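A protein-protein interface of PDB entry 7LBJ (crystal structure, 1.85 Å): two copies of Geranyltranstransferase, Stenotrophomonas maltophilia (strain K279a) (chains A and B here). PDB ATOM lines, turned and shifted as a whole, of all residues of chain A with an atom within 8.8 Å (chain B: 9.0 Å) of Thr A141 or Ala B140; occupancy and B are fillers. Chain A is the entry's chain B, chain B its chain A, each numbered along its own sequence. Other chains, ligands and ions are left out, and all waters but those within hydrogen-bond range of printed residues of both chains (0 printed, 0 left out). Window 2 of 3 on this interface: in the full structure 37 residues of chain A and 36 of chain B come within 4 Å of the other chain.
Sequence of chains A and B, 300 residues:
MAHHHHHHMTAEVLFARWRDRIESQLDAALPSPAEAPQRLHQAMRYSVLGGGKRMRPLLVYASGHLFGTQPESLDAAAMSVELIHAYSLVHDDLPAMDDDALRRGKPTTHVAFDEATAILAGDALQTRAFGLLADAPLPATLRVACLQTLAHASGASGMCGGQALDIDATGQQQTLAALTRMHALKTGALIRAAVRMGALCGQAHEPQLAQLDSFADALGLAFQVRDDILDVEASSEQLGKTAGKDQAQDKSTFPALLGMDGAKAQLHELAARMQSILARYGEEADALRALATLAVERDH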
ATOM      1  N   ALA A 134      11.007   1.683  13.362  1.00  0.00           N
ATOM      2  CA  ALA A 134      10.457   1.145  12.123  1.00  0.00           C
ATOM      3  C   ALA A 134      10.564   2.142  10.969  1.00  0.00           C
ATOM      4  O   ALA A 134      10.701   1.736   9.808  1.00  0.00           O
ATOM      5  CB  ALA A 134       8.997   0.726  12.341  1.00  0.00           C
ATOM      6  N   LEU A 138      17.325   3.556   7.700  1.00  0.00           N
ATOM      7  CA  LEU A 138      18.308   2.497   7.852  1.00  0.00           C
ATOM      8  C   LEU A 138      17.828   1.283   7.077  1.00  0.00           C
ATOM      9  O   LEU A 138      16.623   1.125   6.851  1.00  0.00           O
ATOM     10  CB  LEU A 138      18.488   2.126   9.331  1.00  0.00           C
ATOM     11  CG  LEU A 138      18.916   3.276  10.246  1.00  0.00           C
ATOM     12  CD1 LEU A 138      18.812   2.874  11.706  1.00  0.00           C
ATOM     13  CD2 LEU A 138      20.329   3.645   9.898  1.00  0.00           C
ATOM     14  N   PRO A 139      18.738   0.392   6.681  1.00  0.00           N
ATOM     15  CA  PRO A 139      18.309  -0.864   6.053  1.00  0.00           C
ATOM     16  C   PRO A 139      17.239  -1.568   6.880  1.00  0.00           C
ATOM     17  O   PRO A 139      17.276  -1.564   8.111  1.00  0.00           O
ATOM     18  CB  PRO A 139      19.601  -1.677   5.987  1.00  0.00           C
ATOM     19  CG  PRO A 139      20.683  -0.614   5.854  1.00  0.00           C
ATOM     20  CD  PRO A 139      20.209   0.517   6.725  1.00  0.00           C
ATOM     21  N   ALA A 140      16.262  -2.168   6.188  1.00  0.00           N
ATOM     22  CA  ALA A 140      15.195  -2.875   6.898  1.00  0.00           C
ATOM     23  C   ALA A 140      15.747  -3.998   7.778  1.00  0.00           C
ATOM     24  O   ALA A 140      15.220  -4.249   8.871  1.00  0.00           O
ATOM     25  CB  ALA A 140      14.178  -3.443   5.906  1.00  0.00           C
ATOM     26  N   THR A 141      16.792  -4.702   7.323  1.00  0.00           N
ATOM     27  CA  THR A 141      17.344  -5.770   8.165  1.00  0.00           C
ATOM     28  C   THR A 141      17.890  -5.203   9.469  1.00  0.00           C
ATOM     29  O   THR A 141      17.758  -5.828  10.530  1.00  0.00           O
ATOM     30  CB  THR A 141      18.439  -6.558   7.440  1.00  0.00           C
ATOM     31  OG1 THR A 141      19.461  -5.659   6.979  1.00  0.00           O
ATOM     32  CG2 THR A 141      17.870  -7.364   6.273  1.00  0.00           C
ATOM     33  N   LEU A 142      18.510  -4.027   9.410  1.00  0.00           N
ATOM     34  CA  LEU A 142      19.013  -3.397  10.625  1.00  0.00           C
ATOM     35  C   LEU A 142      17.876  -2.888  11.498  1.00  0.00           C
ATOM     36  O   LEU A 142      17.921  -3.034  12.729  1.00  0.00           O
ATOM     37  CB  LEU A 142      19.974  -2.260  10.265  1.00  0.00           C
ATOM     38  CG  LEU A 142      20.425  -1.380  11.433  1.00  0.00           C
ATOM     39  CD1 LEU A 142      21.197  -2.217  12.449  1.00  0.00           C
ATOM     40  CD2 LEU A 142      21.287  -0.219  10.933  1.00  0.00           C
ATOM     41  N   ARG A 143      16.843  -2.283  10.891  1.00  0.00           N
ATOM     42  CA  ARG A 143      15.695  -1.857  11.686  1.00  0.00           C
ATOM     43  C   ARG A 143      15.067  -3.041  12.411  1.00  0.00           C
ATOM     44  O   ARG A 143      14.734  -2.953  13.601  1.00  0.00           O
ATOM     45  CB  ARG A 143      14.653  -1.161  10.802  1.00  0.00           C
ATOM     46  CG  ARG A 143      15.070   0.248  10.372  1.00  0.00           C
ATOM     47  CD  ARG A 143      14.007   0.889   9.514  1.00  0.00           C
ATOM     48  NE  ARG A 143      14.226   0.586   8.110  1.00  0.00           N
ATOM     49  CZ  ARG A 143      13.370   0.872   7.145  1.00  0.00           C
ATOM     50  NH1 ARG A 143      12.177   1.381   7.409  1.00  0.00           N
ATOM     51  NH2 ARG A 143      13.715   0.637   5.882  1.00  0.00           N
ATOM     52  N   VAL A 144      14.905  -4.161  11.716  1.00  0.00           N
ATOM     53  CA  VAL A 144      14.300  -5.338  12.343  1.00  0.00           C
ATOM     54  C   VAL A 144      15.162  -5.851  13.496  1.00  0.00           C
ATOM     55  O   VAL A 144      14.644  -6.222  14.555  1.00  0.00           O
ATOM     56  CB  VAL A 144      14.053  -6.422  11.281  1.00  0.00           C
ATOM     57  CG1 VAL A 144      13.876  -7.787  11.921  1.00  0.00           C
ATOM     58  CG2 VAL A 144      12.827  -6.041  10.486  1.00  0.00           C
ATOM     59  N   ALA A 145      16.481  -5.884  13.319  1.00  0.00           N
ATOM     60  CA  ALA A 145      17.343  -6.363  14.404  1.00  0.00           C
ATOM     61  C   ALA A 145      17.237  -5.464  15.636  1.00  0.00           C
ATOM     62  O   ALA A 145      17.205  -5.950  16.776  1.00  0.00           O
ATOM     63  CB  ALA A 145      18.794  -6.459  13.924  1.00  0.00           C
ATOM     64  N   CYS A 146      17.162  -4.152  15.429  1.00  0.00           N
ATOM     65  CA  CYS A 146      16.997  -3.244  16.558  1.00  0.00           C
ATOM     66  C   CYS A 146      15.624  -3.402  17.195  1.00  0.00           C
ATOM     67  O   CYS A 146      15.497  -3.373  18.425  1.00  0.00           O
ATOM     68  CB  CYS A 146      17.200  -1.801  16.103  1.00  0.00           C
ATOM     69  SG  CYS A 146      18.915  -1.425  15.677  1.00  0.00           S
ATOM     70  N   LEU A 147      14.584  -3.531  16.376  1.00  0.00           N
ATOM     71  CA  LEU A 147      13.240  -3.715  16.914  1.00  0.00           C
ATOM     72  C   LEU A 147      13.132  -5.016  17.708  1.00  0.00           C
ATOM     73  O   LEU A 147      12.492  -5.059  18.763  1.00  0.00           O
ATOM     74  CB  LEU A 147      12.233  -3.725  15.773  1.00  0.00           C
ATOM     75  CG  LEU A 147      12.010  -2.340  15.171  1.00  0.00           C
ATOM     76  CD1 LEU A 147      11.668  -2.471  13.690  1.00  0.00           C
ATOM     77  CD2 LEU A 147      10.892  -1.680  15.929  1.00  0.00           C
ATOM     78  N   GLN A 148      13.727  -6.095  17.200  1.00  0.00           N
ATOM     79  CA  GLN A 148      13.785  -7.339  17.973  1.00  0.00           C
ATOM     80  C   GLN A 148      14.476  -7.120  19.311  1.00  0.00           C
ATOM     81  O   GLN A 148      14.007  -7.580  20.363  1.00  0.00           O
ATOM     82  CB  GLN A 148      14.539  -8.400  17.177  1.00  0.00           C
ATOM     83  CG  GLN A 148      13.738  -8.975  16.035  1.00  0.00           C
ATOM     84  CD  GLN A 148      14.575  -9.924  15.221  1.00  0.00           C
ATOM     85  OE1 GLN A 148      15.671  -9.575  14.786  1.00  0.00           O
ATOM     86  NE2 GLN A 148      14.102 -11.146  15.069  1.00  0.00           N
ATOM     87  N   LEU A 200      24.968  -2.746  16.658  1.00  0.00           N
ATOM     88  CA  LEU A 200      24.332  -3.175  15.417  1.00  0.00           C
ATOM     89  C   LEU A 200      24.377  -2.075  14.368  1.00  0.00           C
ATOM     90  O   LEU A 200      24.668  -2.334  13.196  1.00  0.00           O
ATOM     91  CB  LEU A 200      22.876  -3.586  15.682  1.00  0.00           C
ATOM     92  CG  LEU A 200      22.674  -4.886  16.472  1.00  0.00           C
ATOM     93  CD1 LEU A 200      21.186  -5.098  16.815  1.00  0.00           C
ATOM     94  CD2 LEU A 200      23.207  -6.089  15.715  1.00  0.00           C
ATOM     95  N   LEU B 133       5.847  -9.278  15.516  1.00  0.00           N
ATOM     96  CA  LEU B 133       6.080  -8.801  14.150  1.00  0.00           C
ATOM     97  C   LEU B 133       7.566  -8.777  13.836  1.00  0.00           C
ATOM     98  O   LEU B 133       7.992  -9.204  12.755  1.00  0.00           O
ATOM     99  CB  LEU B 133       5.487  -7.403  13.936  1.00  0.00           C
ATOM    100  CG  LEU B 133       3.964  -7.241  13.899  1.00  0.00           C
ATOM    101  CD1 LEU B 133       3.588  -5.758  13.699  1.00  0.00           C
ATOM    102  CD2 LEU B 133       3.355  -8.148  12.816  1.00  0.00           C
ATOM    103  N   ALA B 134       8.370  -8.229  14.745  1.00  0.00           N
ATOM    104  CA  ALA B 134       9.800  -8.155  14.462  1.00  0.00           C
ATOM    105  C   ALA B 134      10.411  -9.546  14.311  1.00  0.00           C
ATOM    106  O   ALA B 134      11.407  -9.709  13.593  1.00  0.00           O
ATOM    107  CB  ALA B 134      10.508  -7.352  15.560  1.00  0.00           C
ATOM    108  N   ALA B 136       8.780 -12.230  13.099  1.00  0.00           N
ATOM    109  CA  ALA B 136       8.007 -13.048  12.154  1.00  0.00           C
ATOM    110  C   ALA B 136       8.904 -13.711  11.095  1.00  0.00           C
ATOM    111  O   ALA B 136       9.937 -13.168  10.697  1.00  0.00           O
ATOM    112  CB  ALA B 136       6.934 -12.202  11.470  1.00  0.00           C
ATOM    113  N   PRO B 137       8.525 -14.899  10.608  1.00  0.00           N
ATOM    114  CA  PRO B 137       9.311 -15.567   9.547  1.00  0.00           C
ATOM    115  C   PRO B 137       8.978 -15.020   8.157  1.00  0.00           C
ATOM    116  O   PRO B 137       8.520 -15.733   7.264  1.00  0.00           O
ATOM    117  CB  PRO B 137       8.911 -17.041   9.723  1.00  0.00           C
ATOM    118  CG  PRO B 137       7.490 -16.981  10.208  1.00  0.00           C
ATOM    119  CD  PRO B 137       7.379 -15.710  11.061  1.00  0.00           C
ATOM    120  N   LEU B 138       9.203 -13.728   7.975  1.00  0.00           N
ATOM    121  CA  LEU B 138       8.878 -12.965   6.780  1.00  0.00           C
ATOM    122  C   LEU B 138      10.100 -12.148   6.391  1.00  0.00           C
ATOM    123  O   LEU B 138      10.948 -11.868   7.244  1.00  0.00           O
ATOM    124  CB  LEU B 138       7.704 -12.014   7.055  1.00  0.00           C
ATOM    125  CG  LEU B 138       6.388 -12.640   7.560  1.00  0.00           C
ATOM    126  CD1 LEU B 138       5.394 -11.548   7.967  1.00  0.00           C
ATOM    127  CD2 LEU B 138       5.814 -13.510   6.477  1.00  0.00           C
ATOM    128  N   PRO B 139      10.198 -11.712   5.124  1.00  0.00           N
ATOM    129  CA  PRO B 139      11.267 -10.777   4.728  1.00  0.00           C
ATOM    130  C   PRO B 139      11.290  -9.533   5.606  1.00  0.00           C
ATOM    131  O   PRO B 139      10.253  -9.037   6.041  1.00  0.00           O
ATOM    132  CB  PRO B 139      10.904 -10.419   3.281  1.00  0.00           C
ATOM    133  CG  PRO B 139      10.131 -11.607   2.786  1.00  0.00           C
ATOM    134  CD  PRO B 139       9.346 -12.080   3.978  1.00  0.00           C
ATOM    135  N   ALA B 140      12.496  -9.013   5.850  1.00  0.00           N
ATOM    136  CA  ALA B 140      12.615  -7.867   6.744  1.00  0.00           C
ATOM    137  C   ALA B 140      11.796  -6.677   6.246  1.00  0.00           C
ATOM    138  O   ALA B 140      11.190  -5.959   7.052  1.00  0.00           O
ATOM    139  CB  ALA B 140      14.089  -7.476   6.906  1.00  0.00           C
ATOM    140  N   THR B 141      11.753  -6.451   4.922  1.00  0.00           N
ATOM    141  CA  THR B 141      10.986  -5.313   4.401  1.00  0.00           C
ATOM    142  C   THR B 141       9.506  -5.447   4.731  1.00  0.00           C
ATOM    143  O   THR B 141       8.831  -4.452   5.027  1.00  0.00           O
ATOM    144  CB  THR B 141      11.158  -5.172   2.884  1.00  0.00           C
ATOM    145  OG1 THR B 141      10.805  -6.406   2.235  1.00  0.00           O
ATOM    146  CG2 THR B 141      12.583  -4.778   2.518  1.00  0.00           C
ATOM    147  N   LEU B 142       8.984  -6.675   4.691  1.00  0.00           N
ATOM    148  CA  LEU B 142       7.589  -6.888   5.053  1.00  0.00           C
ATOM    149  C   LEU B 142       7.371  -6.700   6.550  1.00  0.00           C
ATOM    150  O   LEU B 142       6.382  -6.086   6.961  1.00  0.00           O
ATOM    151  CB  LEU B 142       7.130  -8.279   4.590  1.00  0.00           C
ATOM    152  CG  LEU B 142       5.697  -8.684   4.982  1.00  0.00           C
ATOM    153  CD1 LEU B 142       4.707  -7.632   4.470  1.00  0.00           C
ATOM    154  CD2 LEU B 142       5.323 -10.089   4.454  1.00  0.00           C
ATOM    155  N   ARG B 143       8.271  -7.220   7.391  1.00  0.00           N
ATOM    156  CA  ARG B 143       8.091  -7.008   8.825  1.00  0.00           C
ATOM    157  C   ARG B 143       8.118  -5.528   9.157  1.00  0.00           C
ATOM    158  O   ARG B 143       7.321  -5.057   9.972  1.00  0.00           O
ATOM    159  CB  ARG B 143       9.174  -7.733   9.630  1.00  0.00           C
ATOM    160  CG  ARG B 143       9.029  -9.259   9.662  1.00  0.00           C
ATOM    161  CD  ARG B 143      10.204  -9.854  10.451  1.00  0.00           C
ATOM    162  NE  ARG B 143      11.277 -10.312   9.572  1.00  0.00           N
ATOM    163  CZ  ARG B 143      12.432 -10.814   9.998  1.00  0.00           C
ATOM    164  NH1 ARG B 143      12.759 -10.812  11.283  1.00  0.00           N
ATOM    165  NH2 ARG B 143      13.272 -11.348   9.115  1.00  0.00           N
ATOM    166  N   VAL B 144       9.035  -4.778   8.531  1.00  0.00           N
ATOM    167  CA  VAL B 144       9.113  -3.338   8.782  1.00  0.00           C
ATOM    168  C   VAL B 144       7.826  -2.645   8.357  1.00  0.00           C
ATOM    169  O   VAL B 144       7.308  -1.779   9.074  1.00  0.00           O
ATOM    170  CB  VAL B 144      10.343  -2.734   8.074  1.00  0.00           C
ATOM    171  CG1 VAL B 144      10.176  -1.236   7.865  1.00  0.00           C
ATOM    172  CG2 VAL B 144      11.596  -3.034   8.876  1.00  0.00           C
ATOM    173  N   ALA B 145       7.281  -3.015   7.196  1.00  0.00           N
ATOM    174  CA  ALA B 145       6.048  -2.378   6.736  1.00  0.00           C
ATOM    175  C   ALA B 145       4.884  -2.678   7.679  1.00  0.00           C
ATOM    176  O   ALA B 145       4.031  -1.812   7.925  1.00  0.00           O
ATOM    177  CB  ALA B 145       5.707  -2.839   5.312  1.00  0.00           C
ATOM    178  N   CYS B 146       4.826  -3.907   8.204  1.00  0.00           N
ATOM    179  CA  CYS B 146       3.775  -4.234   9.160  1.00  0.00           C
ATOM    180  C   CYS B 146       3.969  -3.477  10.464  1.00  0.00           C
ATOM    181  O   CYS B 146       2.993  -3.015  11.063  1.00  0.00           O
ATOM    182  CB  CYS B 146       3.746  -5.744   9.416  1.00  0.00           C
ATOM    183  SG  CYS B 146       3.038  -6.643   8.048  1.00  0.00           S
ATOM    184  N   LEU B 147       5.218  -3.383  10.937  1.00  0.00           N
ATOM    185  CA  LEU B 147       5.504  -2.670  12.178  1.00  0.00           C
ATOM    186  C   LEU B 147       5.203  -1.185  12.056  1.00  0.00           C
ATOM    187  O   LEU B 147       4.654  -0.589  12.987  1.00  0.00           O
ATOM    188  CB  LEU B 147       6.959  -2.857  12.589  1.00  0.00           C
ATOM    189  CG  LEU B 147       7.291  -4.197  13.253  1.00  0.00           C
ATOM    190  CD1 LEU B 147       8.692  -4.644  12.870  1.00  0.00           C
ATOM    191  CD2 LEU B 147       7.205  -4.055  14.742  1.00  0.00           C
ATOM    192  N   GLN B 148       5.564  -0.562  10.928  1.00  0.00           N
ATOM    193  CA  GLN B 148       5.186   0.832  10.729  1.00  0.00           C
ATOM    194  C   GLN B 148       3.674   0.988  10.777  1.00  0.00           C
ATOM    195  O   GLN B 148       3.143   1.944  11.374  1.00  0.00           O
ATOM    196  CB  GLN B 148       5.703   1.333   9.382  1.00  0.00           C
ATOM    197  CG  GLN B 148       7.211   1.393   9.233  1.00  0.00           C
ATOM    198  CD  GLN B 148       7.617   1.717   7.809  1.00  0.00           C
ATOM    199  OE1 GLN B 148       7.174   1.068   6.865  1.00  0.00           O
ATOM    200  NE2 GLN B 148       8.437   2.729   7.647  1.00  0.00           N
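NE2 of Gln A148 sits at hydrogen-bond distance from O of Ala B134.
The backbone carbonyl oxygen (O) of Ala A134 is in hydrogen-bond range of the side-chain amide nitrogen (NE2) of Gln B148 (3.3 Å).
The guanidinium group (NH1) of Arg B143 is in hydrogen-bond range of the backbone carbonyl oxygen (O) of Ala B134, 2.9 Å away.
The guanidinium group of Arg B143 lies close to the backbone carbonyl oxygen of Ala B136 (3.3 Å).
The backbone carbonyl oxygen of Leu B138 is in hydrogen-bond range of the guanidinium group of Arg B143, 2.8 Å away.
The guanidinium group (NH1) of Arg A143 lies within hydrogen-bond range of the backbone carbonyl oxygen (O) of Ala A134 (2.8 Å).
The guanidinium group (NE) of Arg A143 is in hydrogen-bond range of the backbone carbonyl oxygen (O) of Leu A138, 2.8 Å away.
Among the printed residues, merely in contact across the chains: Ala A134 with Val B144, Ala A140 with Ala B140, Ala A140 with Thr B141, Ala A140 with Val B144, Thr A141 with Ala B140, Arg A143 with Val B144, Arg A143 with Gln B148, Val A144 with Ala B134, Val A144 with Ala B140, Val A144 with Arg B143, Val A144 with Val B144 and Leu A147 with Leu B147.
Of chain B, only Ala B140 (3.9 Å), Thr B141 (3.98 Å) and Val B144 (3.8 Å) come within 4 Å of Ala A140.
Printed residues of chain B within 4 Å of Thr A141: Ala B140 (3.8 Å).
Of the printed residues of chain B, Val A144 touches Ala B134 (3.5 Å), Ala B140 (3.8 Å), Arg B143 (3.3 Å) and Val B144 (3.6 Å).
Of the printed residues of chain A, Ala B140 touches Ala A140 (3.9 Å), Thr A141 (3.8 Å) and Val A144 (3.8 Å).
Of the printed residues of chain A, Val B144 touches Ala A134 (3.6 Å), Ala A140 (3.8 Å), Arg A143 (3.3 Å) and Val A144 (3.6 Å).
Of the printed residues of chain A, Gln B148 touches Ala A134 (3.3 Å) and Arg A143 (3.98 Å).
The nearest residue of chain A that does not touch Ala B140 is Leu A142 (6.1 Å).
Printed residues of chain B that touch a printed residue of chain A: Ala B134, Ala B140, Thr B141, Arg B143, Val B144, Leu B147 and Gln B148.
Hydrophobic or aromatic side chains of chain A that line the printed part of chain B: Ala A134, Ala A140, Val A144 and Leu A147.
Among the printed residues, 14 pairs touch across the chains.
Among the printed residues, no Asp or Glu carboxylate lies within 4 Å of a Lys or Arg side-chain nitrogen of the other chain.
Ala A134 touches Gln B148, and with the chains exchanged Gln A148 touches Ala B134.
Ala A140 touches Thr B141, and with the chains exchanged Thr A141 touches Ala B140.
Val B144 touches its own counterpart, Val A144.
Leu B147 touches its own counterpart, Leu A147.
Of the 14 pairs that touch across the chains among the printed residues, 13 have their exchanged pair printed and touching as well.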
